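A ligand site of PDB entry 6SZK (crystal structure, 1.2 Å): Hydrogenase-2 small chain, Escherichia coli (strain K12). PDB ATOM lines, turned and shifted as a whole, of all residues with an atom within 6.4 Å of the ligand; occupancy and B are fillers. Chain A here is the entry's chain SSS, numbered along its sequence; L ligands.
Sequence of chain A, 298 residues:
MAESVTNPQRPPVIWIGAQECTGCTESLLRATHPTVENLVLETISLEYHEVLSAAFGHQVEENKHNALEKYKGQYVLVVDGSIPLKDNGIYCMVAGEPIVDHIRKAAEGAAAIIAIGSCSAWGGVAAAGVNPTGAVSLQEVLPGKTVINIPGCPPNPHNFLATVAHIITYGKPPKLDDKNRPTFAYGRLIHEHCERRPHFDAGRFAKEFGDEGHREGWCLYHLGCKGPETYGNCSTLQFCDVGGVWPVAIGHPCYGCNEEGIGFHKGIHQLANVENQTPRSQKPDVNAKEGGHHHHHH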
ATOM      1  N   ILE A 190      -7.341  14.177  25.669  1.00  0.00           N
ATOM      2  CA  ILE A 190      -7.094  12.713  25.703  1.00  0.00           C
ATOM      3  C   ILE A 190      -8.130  11.983  24.824  1.00  0.00           C
ATOM      4  O   ILE A 190      -7.737  11.096  23.994  1.00  0.00           O
ATOM      5  CB  ILE A 190      -7.013  12.175  27.151  1.00  0.00           C
ATOM      6  CG1 ILE A 190      -5.720  12.727  27.845  1.00  0.00           C
ATOM      7  CG2 ILE A 190      -7.069  10.657  27.213  1.00  0.00           C
ATOM      8  CD1 ILE A 190      -5.738  12.522  29.356  1.00  0.00           C
ATOM      9  N   HIS A 191      -9.423  12.348  24.898  1.00  0.00           N
ATOM     10  CA  HIS A 191     -10.487  11.693  24.125  1.00  0.00           C
ATOM     11  C   HIS A 191     -10.365  11.942  22.613  1.00  0.00           C
ATOM     12  O   HIS A 191     -10.990  11.151  21.835  1.00  0.00           O
ATOM     13  CB  HIS A 191     -11.845  12.221  24.684  1.00  0.00           C
ATOM     14  CG  HIS A 191     -13.109  11.693  24.071  1.00  0.00           C
ATOM     15  ND1 HIS A 191     -13.623  10.430  24.346  1.00  0.00           N
ATOM     16  CD2 HIS A 191     -13.991  12.281  23.223  1.00  0.00           C
ATOM     17  CE1 HIS A 191     -14.783  10.291  23.666  1.00  0.00           C
ATOM     18  NE2 HIS A 191     -15.024  11.419  22.947  1.00  0.00           N
ATOM     19  N   GLU A 192      -9.669  12.997  22.217  1.00  0.00           N
ATOM     20  CA  GLU A 192      -9.418  13.250  20.797  1.00  0.00           C
ATOM     21  C   GLU A 192      -8.145  12.513  20.270  1.00  0.00           C
ATOM     22  O   GLU A 192      -7.752  12.742  19.082  1.00  0.00           O
ATOM     23  CB  GLU A 192      -9.409  14.766  20.447  1.00  0.00           C
ATOM     24  CG  GLU A 192     -10.795  15.414  20.691  1.00  0.00           C
ATOM     25  CD  GLU A 192     -11.923  14.790  19.838  1.00  0.00           C
ATOM     26  OE1 GLU A 192     -12.998  14.369  20.381  1.00  0.00           O
ATOM     27  OE2 GLU A 192     -11.719  14.655  18.627  1.00  0.00           O
ATOM     28  N   CYS A 194      -7.618   8.884  21.752  1.00  0.00           N
ATOM     29  CA  CYS A 194      -7.744   7.671  22.599  1.00  0.00           C
ATOM     30  C   CYS A 194      -8.058   6.407  21.763  1.00  0.00           C
ATOM     31  O   CYS A 194      -9.046   6.466  20.965  1.00  0.00           O
ATOM     32  CB  CYS A 194      -8.859   7.872  23.652  1.00  0.00           C
ATOM     33  SG  CYS A 194      -9.031   6.398  24.745  1.00  0.00           S
ATOM     34  N   GLU A 195      -7.341   5.325  21.978  1.00  0.00           N
ATOM     35  CA  GLU A 195      -7.544   4.093  21.251  1.00  0.00           C
ATOM     36  C   GLU A 195      -8.876   3.390  21.538  1.00  0.00           C
ATOM     37  O   GLU A 195      -9.252   2.446  20.777  1.00  0.00           O
ATOM     38  CB  GLU A 195      -6.348   3.123  21.438  1.00  0.00           C
ATOM     39  CG  GLU A 195      -6.185   2.539  22.850  1.00  0.00           C
ATOM     40  CD  GLU A 195      -5.476   3.362  23.939  1.00  0.00           C
ATOM     41  OE1 GLU A 195      -5.252   4.614  23.773  1.00  0.00           O
ATOM     42  OE2 GLU A 195      -5.114   2.717  25.019  1.00  0.00           O
ATOM     43  N   ARG A 196      -9.614   3.836  22.584  1.00  0.00           N
ATOM     44  CA  ARG A 196     -10.945   3.247  22.858  1.00  0.00           C
ATOM     45  C   ARG A 196     -12.082   4.082  22.238  1.00  0.00           C
ATOM     46  O   ARG A 196     -13.266   3.680  22.317  1.00  0.00           O
ATOM     47  CB  ARG A 196     -11.172   3.030  24.353  1.00  0.00           C
ATOM     48  CG  ARG A 196     -10.068   2.164  24.974  1.00  0.00           C
ATOM     49  CD  ARG A 196     -10.394   1.599  26.345  1.00  0.00           C
ATOM     50  NE  ARG A 196      -9.319   0.701  26.764  1.00  0.00           N
ATOM     51  CZ  ARG A 196      -9.411  -0.193  27.733  1.00  0.00           C
ATOM     52  NH1 ARG A 196     -10.505  -0.278  28.483  1.00  0.00           N
ATOM     53  NH2 ARG A 196      -8.386  -0.995  27.994  1.00  0.00           N
ATOM     54  N   ARG A 197     -11.746   5.092  21.440  1.00  0.00           N
ATOM     55  CA  ARG A 197     -12.801   5.881  20.785  1.00  0.00           C
ATOM     56  C   ARG A 197     -13.717   5.027  19.872  1.00  0.00           C
ATOM     57  O   ARG A 197     -14.935   5.302  19.808  1.00  0.00           O
ATOM     58  CB  ARG A 197     -12.174   7.028  19.994  1.00  0.00           C
ATOM     59  CG  ARG A 197     -13.155   7.981  19.250  1.00  0.00           C
ATOM     60  CD  ARG A 197     -14.148   8.676  20.193  1.00  0.00           C
ATOM     61  NE  ARG A 197     -14.965   9.616  19.440  1.00  0.00           N
ATOM     62  CZ  ARG A 197     -14.614  10.892  19.174  1.00  0.00           C
ATOM     63  NH1 ARG A 197     -13.583  11.456  19.799  1.00  0.00           N
ATOM     64  NH2 ARG A 197     -15.314  11.609  18.279  1.00  0.00           N
ATOM     65  N   PRO A 198     -13.219   3.985  19.134  1.00  0.00           N
ATOM     66  CA  PRO A 198     -14.156   3.154  18.353  1.00  0.00           C
ATOM     67  C   PRO A 198     -15.283   2.567  19.238  1.00  0.00           C
ATOM     68  O   PRO A 198     -16.432   2.420  18.734  1.00  0.00           O
ATOM     69  CB  PRO A 198     -13.271   2.073  17.713  1.00  0.00           C
ATOM     70  CG  PRO A 198     -11.846   2.689  17.674  1.00  0.00           C
ATOM     71  CD  PRO A 198     -11.812   3.530  18.939  1.00  0.00           C
ATOM     72  N   PHE A 200     -16.462   3.791  22.175  1.00  0.00           N
ATOM     73  CA  PHE A 200     -17.353   4.952  22.489  1.00  0.00           C
ATOM     74  C   PHE A 200     -18.333   5.127  21.325  1.00  0.00           C
ATOM     75  O   PHE A 200     -19.578   5.279  21.538  1.00  0.00           O
ATOM     76  CB  PHE A 200     -16.493   6.206  22.745  1.00  0.00           C
ATOM     77  CG  PHE A 200     -17.288   7.452  23.059  1.00  0.00           C
ATOM     78  CD1 PHE A 200     -17.728   8.300  22.045  1.00  0.00           C
ATOM     79  CD2 PHE A 200     -17.506   7.867  24.360  1.00  0.00           C
ATOM     80  CE1 PHE A 200     -18.406   9.471  22.321  1.00  0.00           C
ATOM     81  CE2 PHE A 200     -18.232   9.026  24.637  1.00  0.00           C
ATOM     82  CZ  PHE A 200     -18.653   9.885  23.642  1.00  0.00           C
ATOM     83  N   PHE A 205     -19.586  -0.080  26.054  1.00  0.00           N
ATOM     84  CA  PHE A 205     -19.183   0.511  27.333  1.00  0.00           C
ATOM     85  C   PHE A 205     -19.035  -0.567  28.423  1.00  0.00           C
ATOM     86  O   PHE A 205     -19.956  -1.377  28.609  1.00  0.00           O
ATOM     87  CB  PHE A 205     -20.200   1.584  27.815  1.00  0.00           C
ATOM     88  CG  PHE A 205     -20.350   2.740  26.864  1.00  0.00           C
ATOM     89  CD1 PHE A 205     -19.313   3.640  26.656  1.00  0.00           C
ATOM     90  CD2 PHE A 205     -21.565   2.958  26.241  1.00  0.00           C
ATOM     91  CE1 PHE A 205     -19.491   4.769  25.875  1.00  0.00           C
ATOM     92  CE2 PHE A 205     -21.744   4.091  25.469  1.00  0.00           C
ATOM     93  CZ  PHE A 205     -20.704   4.977  25.234  1.00  0.00           C
ATOM     94  N   TRP A 218     -13.301  -2.374  26.457  1.00  0.00           N
ATOM     95  CA  TRP A 218     -14.264  -1.377  25.930  1.00  0.00           C
ATOM     96  C   TRP A 218     -14.069   0.003  26.602  1.00  0.00           C
ATOM     97  O   TRP A 218     -13.266   0.208  27.559  1.00  0.00           O
ATOM     98  CB  TRP A 218     -15.686  -1.910  26.096  1.00  0.00           C
ATOM     99  CG  TRP A 218     -16.083  -3.018  25.169  1.00  0.00           C
ATOM    100  CD1 TRP A 218     -15.306  -3.663  24.232  1.00  0.00           C
ATOM    101  CD2 TRP A 218     -17.368  -3.709  25.093  1.00  0.00           C
ATOM    102  NE1 TRP A 218     -16.038  -4.657  23.605  1.00  0.00           N
ATOM    103  CE2 TRP A 218     -17.300  -4.661  24.090  1.00  0.00           C
ATOM    104  CE3 TRP A 218     -18.587  -3.520  25.777  1.00  0.00           C
ATOM    105  CZ2 TRP A 218     -18.423  -5.425  23.719  1.00  0.00           C
ATOM    106  CZ3 TRP A 218     -19.692  -4.263  25.442  1.00  0.00           C
ATOM    107  CH2 TRP A 218     -19.591  -5.221  24.435  1.00  0.00           C
ATOM    108  N   CYS A 219     -14.773   0.993  26.050  1.00  0.00           N
ATOM    109  CA  CYS A 219     -14.641   2.434  26.525  1.00  0.00           C
ATOM    110  C   CYS A 219     -15.107   2.522  28.003  1.00  0.00           C
ATOM    111  O   CYS A 219     -16.068   1.836  28.437  1.00  0.00           O
ATOM    112  CB  CYS A 219     -15.454   3.377  25.577  1.00  0.00           C
ATOM    113  SG  CYS A 219     -15.699   5.072  26.217  1.00  0.00           S
ATOM    114  N   LEU A 220     -14.415   3.395  28.769  1.00  0.00           N
ATOM    115  CA  LEU A 220     -14.616   3.636  30.208  1.00  0.00           C
ATOM    116  C   LEU A 220     -15.486   4.880  30.515  1.00  0.00           C
ATOM    117  O   LEU A 220     -15.570   5.297  31.705  1.00  0.00           O
ATOM    118  CB  LEU A 220     -13.277   3.635  30.936  1.00  0.00           C
ATOM    119  CG  LEU A 220     -12.361   2.447  30.616  1.00  0.00           C
ATOM    120  CD1 LEU A 220     -11.110   2.481  31.531  1.00  0.00           C
ATOM    121  CD2 LEU A 220     -13.070   1.088  30.840  1.00  0.00           C
ATOM    122  N   TYR A 221     -16.133   5.476  29.519  1.00  0.00           N
ATOM    123  CA  TYR A 221     -16.965   6.690  29.698  1.00  0.00           C
ATOM    124  C   TYR A 221     -17.951   6.538  30.859  1.00  0.00           C
ATOM    125  O   TYR A 221     -18.068   7.470  31.742  1.00  0.00           O
ATOM    126  CB  TYR A 221     -17.687   7.123  28.427  1.00  0.00           C
ATOM    127  CG  TYR A 221     -18.542   8.381  28.626  1.00  0.00           C
ATOM    128  CD1 TYR A 221     -17.941   9.623  28.735  1.00  0.00           C
ATOM    129  CD2 TYR A 221     -19.913   8.302  28.833  1.00  0.00           C
ATOM    130  CE1 TYR A 221     -18.661  10.776  28.981  1.00  0.00           C
ATOM    131  CE2 TYR A 221     -20.673   9.429  29.111  1.00  0.00           C
ATOM    132  CZ  TYR A 221     -20.038  10.682  29.229  1.00  0.00           C
ATOM    133  OH  TYR A 221     -20.783  11.822  29.548  1.00  0.00           O
ATOM    134  N   HIS A 222     -18.735   5.448  30.877  1.00  0.00           N
ATOM    135  CA  HIS A 222     -19.797   5.240  31.889  1.00  0.00           C
ATOM    136  C   HIS A 222     -19.241   4.789  33.253  1.00  0.00           C
ATOM    137  O   HIS A 222     -20.042   4.698  34.198  1.00  0.00           O
ATOM    138  CB  HIS A 222     -20.928   4.331  31.331  1.00  0.00           C
ATOM    139  CG  HIS A 222     -21.837   5.098  30.421  1.00  0.00           C
ATOM    140  ND1 HIS A 222     -22.790   5.983  30.906  1.00  0.00           N
ATOM    141  CD2 HIS A 222     -21.951   5.085  29.054  1.00  0.00           C
ATOM    142  CE1 HIS A 222     -23.419   6.546  29.884  1.00  0.00           C
ATOM    143  NE2 HIS A 222     -22.889   6.055  28.703  1.00  0.00           N
ATOM    144  N   CYS A 225     -14.851   8.244  33.021  1.00  0.00           N
ATOM    145  CA  CYS A 225     -13.638   8.710  32.333  1.00  0.00           C
ATOM    146  C   CYS A 225     -13.731  10.241  32.009  1.00  0.00           C
ATOM    147  O   CYS A 225     -14.682  10.719  31.370  1.00  0.00           O
ATOM    148  CB  CYS A 225     -13.395   7.913  31.043  1.00  0.00           C
ATOM    149  SG  CYS A 225     -11.794   8.296  30.283  1.00  0.00           S
ATOM    150  N   LYS A 226     -12.665  10.947  32.428  1.00  0.00           N
ATOM    151  CA  LYS A 226     -12.547  12.405  32.199  1.00  0.00           C
ATOM    152  C   LYS A 226     -11.738  12.764  30.956  1.00  0.00           C
ATOM    153  O   LYS A 226     -11.476  13.971  30.682  1.00  0.00           O
ATOM    154  CB  LYS A 226     -12.030  13.128  33.443  1.00  0.00           C
ATOM    155  CG  LYS A 226     -12.818  12.860  34.721  1.00  0.00           C
ATOM    156  CD  LYS A 226     -14.319  13.111  34.616  1.00  0.00           C
ATOM    157  CE  LYS A 226     -15.100  13.112  35.935  1.00  0.00           C
ATOM    158  NZ  LYS A 226     -14.855  11.797  36.673  1.00  0.00           N
ATOM    159  N   GLY A 227     -11.364  11.768  30.135  1.00  0.00           N
ATOM    160  CA  GLY A 227     -10.690  12.058  28.856  1.00  0.00           C
ATOM    161  C   GLY A 227     -11.370  13.105  27.960  1.00  0.00           C
ATOM    162  O   GLY A 227     -10.668  13.932  27.344  1.00  0.00           O
ATOM    163  N   PRO A 228     -12.718  13.172  27.934  1.00  0.00           N
ATOM    164  CA  PRO A 228     -13.369  14.196  27.099  1.00  0.00           C
ATOM    165  C   PRO A 228     -13.134  15.648  27.499  1.00  0.00           C
ATOM    166  O   PRO A 228     -13.442  16.583  26.737  1.00  0.00           O
ATOM    167  CB  PRO A 228     -14.885  13.847  27.170  1.00  0.00           C
ATOM    168  CG  PRO A 228     -14.860  12.339  27.417  1.00  0.00           C
ATOM    169  CD  PRO A 228     -13.676  12.142  28.389  1.00  0.00           C
ATOM    170  N   TRP A 246      -0.958   3.157  30.729  1.00  0.00           N
ATOM    171  CA  TRP A 246      -1.615   4.400  31.208  1.00  0.00           C
ATOM    172  C   TRP A 246      -2.879   3.970  31.893  1.00  0.00           C
ATOM    173  O   TRP A 246      -3.309   2.764  31.808  1.00  0.00           O
ATOM    174  CB  TRP A 246      -1.848   5.457  30.084  1.00  0.00           C
ATOM    175  CG  TRP A 246      -2.902   5.153  29.037  1.00  0.00           C
ATOM    176  CD1 TRP A 246      -2.860   4.222  27.998  1.00  0.00           C
ATOM    177  CD2 TRP A 246      -4.119   5.921  28.784  1.00  0.00           C
ATOM    178  NE1 TRP A 246      -3.955   4.372  27.152  1.00  0.00           N
ATOM    179  CE2 TRP A 246      -4.741   5.390  27.609  1.00  0.00           C
ATOM    180  CE3 TRP A 246      -4.730   7.043  29.444  1.00  0.00           C
ATOM    181  CZ2 TRP A 246      -5.935   5.952  27.069  1.00  0.00           C
ATOM    182  CZ3 TRP A 246      -5.858   7.573  28.906  1.00  0.00           C
ATOM    183  CH2 TRP A 246      -6.440   7.053  27.718  1.00  0.00           C
ATOM    184  N   VAL A 248      -6.218   4.185  31.614  1.00  0.00           N
ATOM    185  CA  VAL A 248      -7.324   3.594  30.802  1.00  0.00           C
ATOM    186  C   VAL A 248      -6.882   2.225  30.264  1.00  0.00           C
ATOM    187  O   VAL A 248      -7.639   1.228  30.304  1.00  0.00           O
ATOM    188  CB  VAL A 248      -7.767   4.547  29.699  1.00  0.00           C
ATOM    189  CG1 VAL A 248      -8.616   3.838  28.625  1.00  0.00           C
ATOM    190  CG2 VAL A 248      -8.577   5.714  30.268  1.00  0.00           C
ATOM    191  N   PRO A 253     -10.832   4.514  34.592  1.00  0.00           N
ATOM    192  CA  PRO A 253     -11.048   5.807  33.914  1.00  0.00           C
ATOM    193  C   PRO A 253      -9.947   6.856  34.225  1.00  0.00           C
ATOM    194  O   PRO A 253      -9.382   6.860  35.329  1.00  0.00           O
ATOM    195  CB  PRO A 253     -12.431   6.231  34.434  1.00  0.00           C
ATOM    196  CG  PRO A 253     -12.660   5.471  35.725  1.00  0.00           C
ATOM    197  CD  PRO A 253     -11.999   4.127  35.447  1.00  0.00           C
ATOM    198  N   CYS A 254      -9.712   7.758  33.268  1.00  0.00           N
ATOM    199  CA  CYS A 254      -9.042   9.007  33.597  1.00  0.00           C
ATOM    200  C   CYS A 254      -9.857   9.796  34.647  1.00  0.00           C
ATOM    201  O   CYS A 254     -11.116   9.816  34.564  1.00  0.00           O
ATOM    202  CB  CYS A 254      -8.835   9.864  32.309  1.00  0.00           C
ATOM    203  SG  CYS A 254      -8.175  11.561  32.549  1.00  0.00           S
HETATM  204 FE1  LIG L   1     -13.744   6.299  26.212  1.00  0.00          FE
HETATM  205 FE2  LIG L   1     -12.210   7.797  28.048  1.00  0.00          FE
HETATM  206 FE3  LIG L   1     -12.954   8.872  25.588  1.00  0.00          FE
HETATM  207 FE4  LIG L   1     -11.084   6.892  25.709  1.00  0.00          FE
HETATM  208  S1  LIG L   1     -10.886   9.075  26.596  1.00  0.00           S
HETATM  209  S2  LIG L   1     -12.852   6.982  24.196  1.00  0.00           S
HETATM  210  S3  LIG L   1     -11.907   5.534  27.418  1.00  0.00           S
HETATM  211  S4  LIG L   1     -14.366   8.296  27.331  1.00  0.00           S
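Arg 196 touches the ligand (C to S2, 3.6 Å).
Phe 200 touches the ligand (CB to S2, 3.996 Å).
Tyr 221 touches the ligand (CB to S4, 3.7 Å).
Gly 227 touches the ligand.
CG1 of Val 248 touches S3 of the ligand, at 3.9 Å.
Hydrophobic or aromatic side chains within 4 Å of the ligand: His 191, Phe 200, Tyr 221 and Val 248.
The nearest printed residue that does not touch the ligand is Pro 228 (4.05 Å).
The backbone carbonyl oxygen (O) of His 191 sits at hydrogen-bond distance from the guanidinium group (NH1) of Arg 197, 3.3 Å away.
The backbone NH of Tyr 221 sits close to the side-chain sulfur of Cys 219.
The side-chain sulfur (SG) of Cys 194 lies close to the backbone NH (N) of Arg 196, 3.4 Å away.
The backbone NH (N) of Cys 225 sits at hydrogen-bond distance from the backbone carbonyl oxygen (O) of Leu 220, 3.3 Å away.
SG of Cys 225 lies close to N of Gly 227 (3.5 Å).
The side-chain sulfur (SG) of Cys 225 sits close to the backbone NH (N) of Cys 254, at 3.7 Å.
The side-chain carboxylate (OE1) of Glu 192 lies within salt-bridge range of the guanidinium group (NH1) of Arg 197 (3.0 Å).
The guanidinium group (NH2) of Arg 196 is in hydrogen-bond range of the backbone carbonyl oxygen (O) of Val 248, at 3.3 Å.
A ring nitrogen (ND1) of His 191 is bound to an iron atom (FE3) of the ligand (2.1 Å).
An iron atom (FE1) of the ligand is bound by the side-chain sulfur (SG) of Cys 219 (2.3 Å).
FE4 of the ligand is bound by SG of Cys 194, at 2.3 Å.
SG of Cys 225 binds FE2 of the ligand.
The backbone NH of Arg 197 lies close to a sulfur (S2) of the ligand, at 3.5 Å.
S3 of the ligand lies close to N of Leu 220 (3.6 Å).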
